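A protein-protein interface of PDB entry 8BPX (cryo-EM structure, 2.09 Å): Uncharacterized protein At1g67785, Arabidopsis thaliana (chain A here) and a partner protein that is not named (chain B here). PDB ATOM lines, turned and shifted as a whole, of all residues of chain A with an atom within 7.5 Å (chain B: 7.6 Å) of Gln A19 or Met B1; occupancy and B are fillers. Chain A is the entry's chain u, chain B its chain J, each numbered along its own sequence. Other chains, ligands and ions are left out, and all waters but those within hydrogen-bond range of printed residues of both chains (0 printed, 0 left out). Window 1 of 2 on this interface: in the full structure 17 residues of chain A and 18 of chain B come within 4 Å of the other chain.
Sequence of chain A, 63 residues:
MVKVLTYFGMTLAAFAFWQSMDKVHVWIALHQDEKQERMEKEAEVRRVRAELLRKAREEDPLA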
ATOM      1  N   LEU A  12       5.930  11.367  -3.679  1.00  0.00           N
ATOM      2  CA  LEU A  12       6.666  10.669  -4.738  1.00  0.00           C
ATOM      3  C   LEU A  12       5.719  10.064  -5.771  1.00  0.00           C
ATOM      4  O   LEU A  12       5.954  10.164  -6.986  1.00  0.00           O
ATOM      5  CB  LEU A  12       7.547   9.576  -4.134  1.00  0.00           C
ATOM      6  CG  LEU A  12       8.723   9.988  -3.253  1.00  0.00           C
ATOM      7  CD1 LEU A  12       9.310   8.764  -2.570  1.00  0.00           C
ATOM      8  CD2 LEU A  12       9.779  10.697  -4.070  1.00  0.00           C
ATOM      9  N   ALA A  13       4.643   9.428  -5.303  1.00  0.00           N
ATOM     10  CA  ALA A  13       3.666   8.859  -6.228  1.00  0.00           C
ATOM     11  C   ALA A  13       3.037   9.943  -7.097  1.00  0.00           C
ATOM     12  O   ALA A  13       2.836   9.751  -8.304  1.00  0.00           O
ATOM     13  CB  ALA A  13       2.591   8.097  -5.455  1.00  0.00           C
ATOM     14  N   ALA A  14       2.729  11.095  -6.499  1.00  0.00           N
ATOM     15  CA  ALA A  14       2.165  12.200  -7.263  1.00  0.00           C
ATOM     16  C   ALA A  14       3.157  12.722  -8.299  1.00  0.00           C
ATOM     17  O   ALA A  14       2.768  13.069  -9.421  1.00  0.00           O
ATOM     18  CB  ALA A  14       1.723  13.315  -6.315  1.00  0.00           C
ATOM     19  N   PHE A  15       4.441  12.789  -7.941  1.00  0.00           N
ATOM     20  CA  PHE A  15       5.454  13.201  -8.908  1.00  0.00           C
ATOM     21  C   PHE A  15       5.480  12.260 -10.107  1.00  0.00           C
ATOM     22  O   PHE A  15       5.540  12.708 -11.265  1.00  0.00           O
ATOM     23  CB  PHE A  15       6.826  13.259  -8.239  1.00  0.00           C
ATOM     24  CG  PHE A  15       7.919  13.732  -9.150  1.00  0.00           C
ATOM     25  CD1 PHE A  15       7.958  15.049  -9.581  1.00  0.00           C
ATOM     26  CD2 PHE A  15       8.893  12.857  -9.599  1.00  0.00           C
ATOM     27  CE1 PHE A  15       8.962  15.483 -10.427  1.00  0.00           C
ATOM     28  CE2 PHE A  15       9.893  13.287 -10.443  1.00  0.00           C
ATOM     29  CZ  PHE A  15       9.926  14.602 -10.861  1.00  0.00           C
ATOM     30  N   ALA A  16       5.414  10.951  -9.845  1.00  0.00           N
ATOM     31  CA  ALA A  16       5.353   9.987 -10.941  1.00  0.00           C
ATOM     32  C   ALA A  16       4.110  10.206 -11.799  1.00  0.00           C
ATOM     33  O   ALA A  16       4.174  10.138 -13.036  1.00  0.00           O
ATOM     34  CB  ALA A  16       5.390   8.561 -10.391  1.00  0.00           C
ATOM     35  N   PHE A  17       2.973  10.484 -11.155  1.00  0.00           N
ATOM     36  CA  PHE A  17       1.739  10.749 -11.893  1.00  0.00           C
ATOM     37  C   PHE A  17       1.889  11.951 -12.822  1.00  0.00           C
ATOM     38  O   PHE A  17       1.429  11.919 -13.970  1.00  0.00           O
ATOM     39  CB  PHE A  17       0.585  10.970 -10.917  1.00  0.00           C
ATOM     40  CG  PHE A  17      -0.595  11.686 -11.519  1.00  0.00           C
ATOM     41  CD1 PHE A  17      -1.497  11.009 -12.327  1.00  0.00           C
ATOM     42  CD2 PHE A  17      -0.807  13.034 -11.271  1.00  0.00           C
ATOM     43  CE1 PHE A  17      -2.583  11.662 -12.879  1.00  0.00           C
ATOM     44  CE2 PHE A  17      -1.889  13.695 -11.820  1.00  0.00           C
ATOM     45  CZ  PHE A  17      -2.781  13.007 -12.625  1.00  0.00           C
ATOM     46  N   TRP A  18       2.520  13.023 -12.341  1.00  0.00           N
ATOM     47  CA  TRP A  18       2.660  14.219 -13.172  1.00  0.00           C
ATOM     48  C   TRP A  18       3.615  13.986 -14.338  1.00  0.00           C
ATOM     49  O   TRP A  18       3.380  14.485 -15.447  1.00  0.00           O
ATOM     50  CB  TRP A  18       3.105  15.414 -12.330  1.00  0.00           C
ATOM     51  CG  TRP A  18       2.029  15.898 -11.421  1.00  0.00           C
ATOM     52  CD1 TRP A  18       1.986  15.780 -10.066  1.00  0.00           C
ATOM     53  CD2 TRP A  18       0.800  16.525 -11.808  1.00  0.00           C
ATOM     54  NE1 TRP A  18       0.824  16.321  -9.580  1.00  0.00           N
ATOM     55  CE2 TRP A  18       0.075  16.782 -10.630  1.00  0.00           C
ATOM     56  CE3 TRP A  18       0.249  16.906 -13.035  1.00  0.00           C
ATOM     57  CZ2 TRP A  18      -1.171  17.404 -10.639  1.00  0.00           C
ATOM     58  CZ3 TRP A  18      -0.991  17.524 -13.044  1.00  0.00           C
ATOM     59  CH2 TRP A  18      -1.686  17.767 -11.853  1.00  0.00           C
ATOM     60  N   GLN A  19       4.691  13.226 -14.123  1.00  0.00           N
ATOM     61  CA  GLN A  19       5.557  12.889 -15.255  1.00  0.00           C
ATOM     62  C   GLN A  19       4.808  12.050 -16.296  1.00  0.00           C
ATOM     63  O   GLN A  19       4.965  12.253 -17.512  1.00  0.00           O
ATOM     64  CB  GLN A  19       6.816  12.179 -14.763  1.00  0.00           C
ATOM     65  CG  GLN A  19       7.550  12.910 -13.639  1.00  0.00           C
ATOM     66  CD  GLN A  19       8.223  14.200 -14.088  1.00  0.00           C
ATOM     67  OE1 GLN A  19       7.561  15.200 -14.359  1.00  0.00           O
ATOM     68  NE2 GLN A  19       9.547  14.186 -14.146  1.00  0.00           N
ATOM     69  N   SER A  20       3.965  11.120 -15.838  1.00  0.00           N
ATOM     70  CA  SER A  20       3.128  10.366 -16.769  1.00  0.00           C
ATOM     71  C   SER A  20       2.190  11.288 -17.544  1.00  0.00           C
ATOM     72  O   SER A  20       1.974  11.105 -18.751  1.00  0.00           O
ATOM     73  CB  SER A  20       2.327   9.304 -16.015  1.00  0.00           C
ATOM     74  OG  SER A  20       3.095   8.720 -14.982  1.00  0.00           O
ATOM     75  N   MET A  21       1.610  12.274 -16.860  1.00  0.00           N
ATOM     76  CA  MET A  21       0.754  13.245 -17.535  1.00  0.00           C
ATOM     77  C   MET A  21       1.531  13.999 -18.609  1.00  0.00           C
ATOM     78  O   MET A  21       0.994  14.301 -19.682  1.00  0.00           O
ATOM     79  CB  MET A  21       0.166  14.220 -16.515  1.00  0.00           C
ATOM     80  CG  MET A  21      -1.177  13.804 -15.916  1.00  0.00           C
ATOM     81  SD  MET A  21      -2.331  13.019 -17.061  1.00  0.00           S
ATOM     82  CE  MET A  21      -2.053  11.285 -16.703  1.00  0.00           C
ATOM     83  N   ASP A  22       2.795  14.320 -18.328  1.00  0.00           N
ATOM     84  CA  ASP A  22       3.646  14.955 -19.331  1.00  0.00           C
ATOM     85  C   ASP A  22       3.770  14.081 -20.574  1.00  0.00           C
ATOM     86  O   ASP A  22       3.670  14.568 -21.711  1.00  0.00           O
ATOM     87  CB  ASP A  22       5.030  15.232 -18.745  1.00  0.00           C
ATOM     88  CG  ASP A  22       5.043  16.416 -17.803  1.00  0.00           C
ATOM     89  OD1 ASP A  22       3.965  16.801 -17.307  1.00  0.00           O
ATOM     90  OD2 ASP A  22       6.139  16.963 -17.557  1.00  0.00           O
ATOM     91  N   LYS A  23       4.005  12.784 -20.370  1.00  0.00           N
ATOM     92  CA  LYS A  23       4.072  11.866 -21.508  1.00  0.00           C
ATOM     93  C   LYS A  23       2.763  11.867 -22.292  1.00  0.00           C
ATOM     94  O   LYS A  23       2.767  11.824 -23.530  1.00  0.00           O
ATOM     95  CB  LYS A  23       4.406  10.453 -21.036  1.00  0.00           C
ATOM     96  CG  LYS A  23       5.804  10.300 -20.478  1.00  0.00           C
ATOM     97  CD  LYS A  23       6.033   8.896 -19.956  1.00  0.00           C
ATOM     98  CE  LYS A  23       7.513   8.616 -19.762  1.00  0.00           C
ATOM     99  NZ  LYS A  23       8.357   9.560 -20.544  1.00  0.00           N
ATOM    100  N   VAL A  24       1.632  11.917 -21.582  1.00  0.00           N
ATOM    101  CA  VAL A  24       0.328  11.962 -22.247  1.00  0.00           C
ATOM    102  C   VAL A  24       0.206  13.212 -23.113  1.00  0.00           C
ATOM    103  O   VAL A  24      -0.300  13.157 -24.244  1.00  0.00           O
ATOM    104  CB  VAL A  24      -0.809  11.885 -21.211  1.00  0.00           C
ATOM    105  CG1 VAL A  24      -2.155  12.079 -21.890  1.00  0.00           C
ATOM    106  CG2 VAL A  24      -0.774  10.557 -20.477  1.00  0.00           C
ATOM    107  N   HIS A  25       0.632  14.360 -22.585  1.00  0.00           N
ATOM    108  CA  HIS A  25       0.543  15.597 -23.357  1.00  0.00           C
ATOM    109  C   HIS A  25       1.409  15.526 -24.608  1.00  0.00           C
ATOM    110  O   HIS A  25       1.002  15.993 -25.681  1.00  0.00           O
ATOM    111  CB  HIS A  25       0.933  16.794 -22.491  1.00  0.00           C
ATOM    112  CG  HIS A  25       0.006  17.031 -21.340  1.00  0.00           C
ATOM    113  ND1 HIS A  25      -1.361  17.116 -21.494  1.00  0.00           N
ATOM    114  CD2 HIS A  25       0.247  17.196 -20.019  1.00  0.00           C
ATOM    115  CE1 HIS A  25      -1.922  17.318 -20.316  1.00  0.00           C
ATOM    116  NE2 HIS A  25      -0.967  17.376 -19.405  1.00  0.00           N
ATOM    117  N   MET B   1       9.388  20.172 -14.340  1.00  0.00           N
ATOM    118  CA  MET B   1       9.995  19.446 -13.231  1.00  0.00           C
ATOM    119  C   MET B   1       9.696  20.153 -11.912  1.00  0.00           C
ATOM    120  O   MET B   1       9.169  19.544 -10.984  1.00  0.00           O
ATOM    121  CB  MET B   1      11.505  19.305 -13.441  1.00  0.00           C
ATOM    122  CG  MET B   1      12.247  18.581 -12.327  1.00  0.00           C
ATOM    123  SD  MET B   1      11.806  16.841 -12.212  1.00  0.00           S
ATOM    124  CE  MET B   1      12.812  16.327 -10.822  1.00  0.00           C
ATOM    125  N   ILE B   2      10.035  21.443 -11.836  1.00  0.00           N
ATOM    126  CA  ILE B   2       9.684  22.230 -10.658  1.00  0.00           C
ATOM    127  C   ILE B   2       8.171  22.326 -10.538  1.00  0.00           C
ATOM    128  O   ILE B   2       7.604  22.199  -9.443  1.00  0.00           O
ATOM    129  CB  ILE B   2      10.341  23.619 -10.727  1.00  0.00           C
ATOM    130  CG1 ILE B   2      11.839  23.509 -10.438  1.00  0.00           C
ATOM    131  CG2 ILE B   2       9.673  24.577  -9.746  1.00  0.00           C
ATOM    132  CD1 ILE B   2      12.476  24.795  -9.961  1.00  0.00           C
ATOM    133  N   LEU B   3       7.482  22.486 -11.655  1.00  0.00           N
ATOM    134  CA  LEU B   3       6.000  22.478 -11.652  1.00  0.00           C
ATOM    135  C   LEU B   3       5.467  21.081 -11.336  1.00  0.00           C
ATOM    136  O   LEU B   3       4.372  20.976 -10.890  1.00  0.00           O
ATOM    137  CB  LEU B   3       5.455  22.974 -12.998  1.00  0.00           C
ATOM    138  CG  LEU B   3       5.617  24.454 -13.302  1.00  0.00           C
ATOM    139  CD1 LEU B   3       5.523  24.693 -14.801  1.00  0.00           C
ATOM    140  CD2 LEU B   3       4.552  25.247 -12.564  1.00  0.00           C
ATOM    141  N   SER B   4       6.232  20.062 -11.666  1.00  0.00           N
ATOM    142  CA  SER B   4       5.844  18.732 -11.212  1.00  0.00           C
ATOM    143  C   SER B   4       5.935  18.619  -9.693  1.00  0.00           C
ATOM    144  O   SER B   4       5.033  18.070  -9.055  1.00  0.00           O
ATOM    145  CB  SER B   4       6.706  17.669 -11.891  1.00  0.00           C
ATOM    146  OG  SER B   4       6.225  17.383 -13.192  1.00  0.00           O
ATOM    147  N   VAL B   5       7.005  19.155  -9.097  1.00  0.00           N
ATOM    148  CA  VAL B   5       7.161  19.102  -7.643  1.00  0.00           C
ATOM    149  C   VAL B   5       6.038  19.869  -6.953  1.00  0.00           C
ATOM    150  O   VAL B   5       5.393  19.362  -6.024  1.00  0.00           O
ATOM    151  CB  VAL B   5       8.542  19.642  -7.228  1.00  0.00           C
ATOM    152  CG1 VAL B   5       8.658  19.685  -5.713  1.00  0.00           C
ATOM    153  CG2 VAL B   5       9.651  18.784  -7.814  1.00  0.00           C
ATOM    154  N   LEU B   6       5.799  21.111  -7.386  1.00  0.00           N
ATOM    155  CA  LEU B   6       4.770  21.917  -6.737  1.00  0.00           C
ATOM    156  C   LEU B   6       3.383  21.315  -6.935  1.00  0.00           C
ATOM    157  O   LEU B   6       2.571  21.305  -6.004  1.00  0.00           O
ATOM    158  CB  LEU B   6       4.823  23.366  -7.229  1.00  0.00           C
ATOM    159  CG  LEU B   6       6.092  24.150  -6.873  1.00  0.00           C
ATOM    160  CD1 LEU B   6       5.990  25.607  -7.294  1.00  0.00           C
ATOM    161  CD2 LEU B   6       6.403  24.051  -5.387  1.00  0.00           C
ATOM    162  N   SER B   7       3.099  20.781  -8.127  1.00  0.00           N
ATOM    163  CA  SER B   7       1.802  20.154  -8.356  1.00  0.00           C
ATOM    164  C   SER B   7       1.636  18.890  -7.523  1.00  0.00           C
ATOM    165  O   SER B   7       0.533  18.602  -7.056  1.00  0.00           O
ATOM    166  CB  SER B   7       1.605  19.846  -9.841  1.00  0.00           C
ATOM    167  OG  SER B   7       1.546  21.025 -10.617  1.00  0.00           O
ATOM    168  N   SER B   8       2.707  18.115  -7.333  1.00  0.00           N
ATOM    169  CA  SER B   8       2.613  16.936  -6.481  1.00  0.00           C
ATOM    170  C   SER B   8       2.334  17.328  -5.033  1.00  0.00           C
ATOM    171  O   SER B   8       1.489  16.715  -4.363  1.00  0.00           O
ATOM    172  CB  SER B   8       3.897  16.114  -6.586  1.00  0.00           C
ATOM    173  OG  SER B   8       4.852  16.528  -5.628  1.00  0.00           O
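Hydrophobic or aromatic side chains of chain B that line the printed part of chain A: Met B1.
Of the 14 printed residues of chain A, 4 touch a printed residue of chain B.
Hydrophobic or aromatic side chains of chain A that line the printed part of chain B: Ala A14, Phe A15 and Trp A18.
Among the printed residues, no Asp or Glu carboxylate lies within 4 Å of a Lys or Arg side-chain nitrogen of the other chain.
Printed residues of chain A within 4 Å of Met B1: Phe A15 (3.2 Å) and Gln A19 (3.99 Å).
Of the printed residues of chain B, Phe A15 touches Met B1, Ser B4 and Ser B8.
Of the printed residues of chain A, Ser B4 touches Phe A15, Trp A18 and Gln A19.
Printed residues of chain B within 4 Å of Trp A18: Ser B4, Ser B7 and Ser B8.
The nearest printed residue of chain B that does not touch Gln A19 is Val B5 (6.6 Å).
OG of Ser B4 sits at hydrogen-bond distance from OE1 of Gln A19 (2.8 Å).
The backbone NH (N) of Ser B8 lies close to the indole nitrogen (NE1) of Trp A18 (3.4 Å).
The backbone carbonyl oxygen (O) of Ser B7 lies close to the indole nitrogen (NE1) of Trp A18, at 3.4 Å.
O of Val B5 sits at hydrogen-bond distance from OG of Ser B8 (2.9 Å).
O of Leu B3 sits at hydrogen-bond distance from OG of Ser B7 (2.8 Å).
CB of Ala A14 touches CB of Ser B8, 3.6 Å away.
SD of Met B1 touches CZ of Phe A15 (3.2 Å).
Phe A15 touches Ser B4.
Phe A15 touches Ser B8 (N to CB, 3.6 Å).
Trp A18 touches Ser B4 (CB to OG, 3.8 Å).
Met B1 touches Gln A19 (SD to NE2, 3.99 Å).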
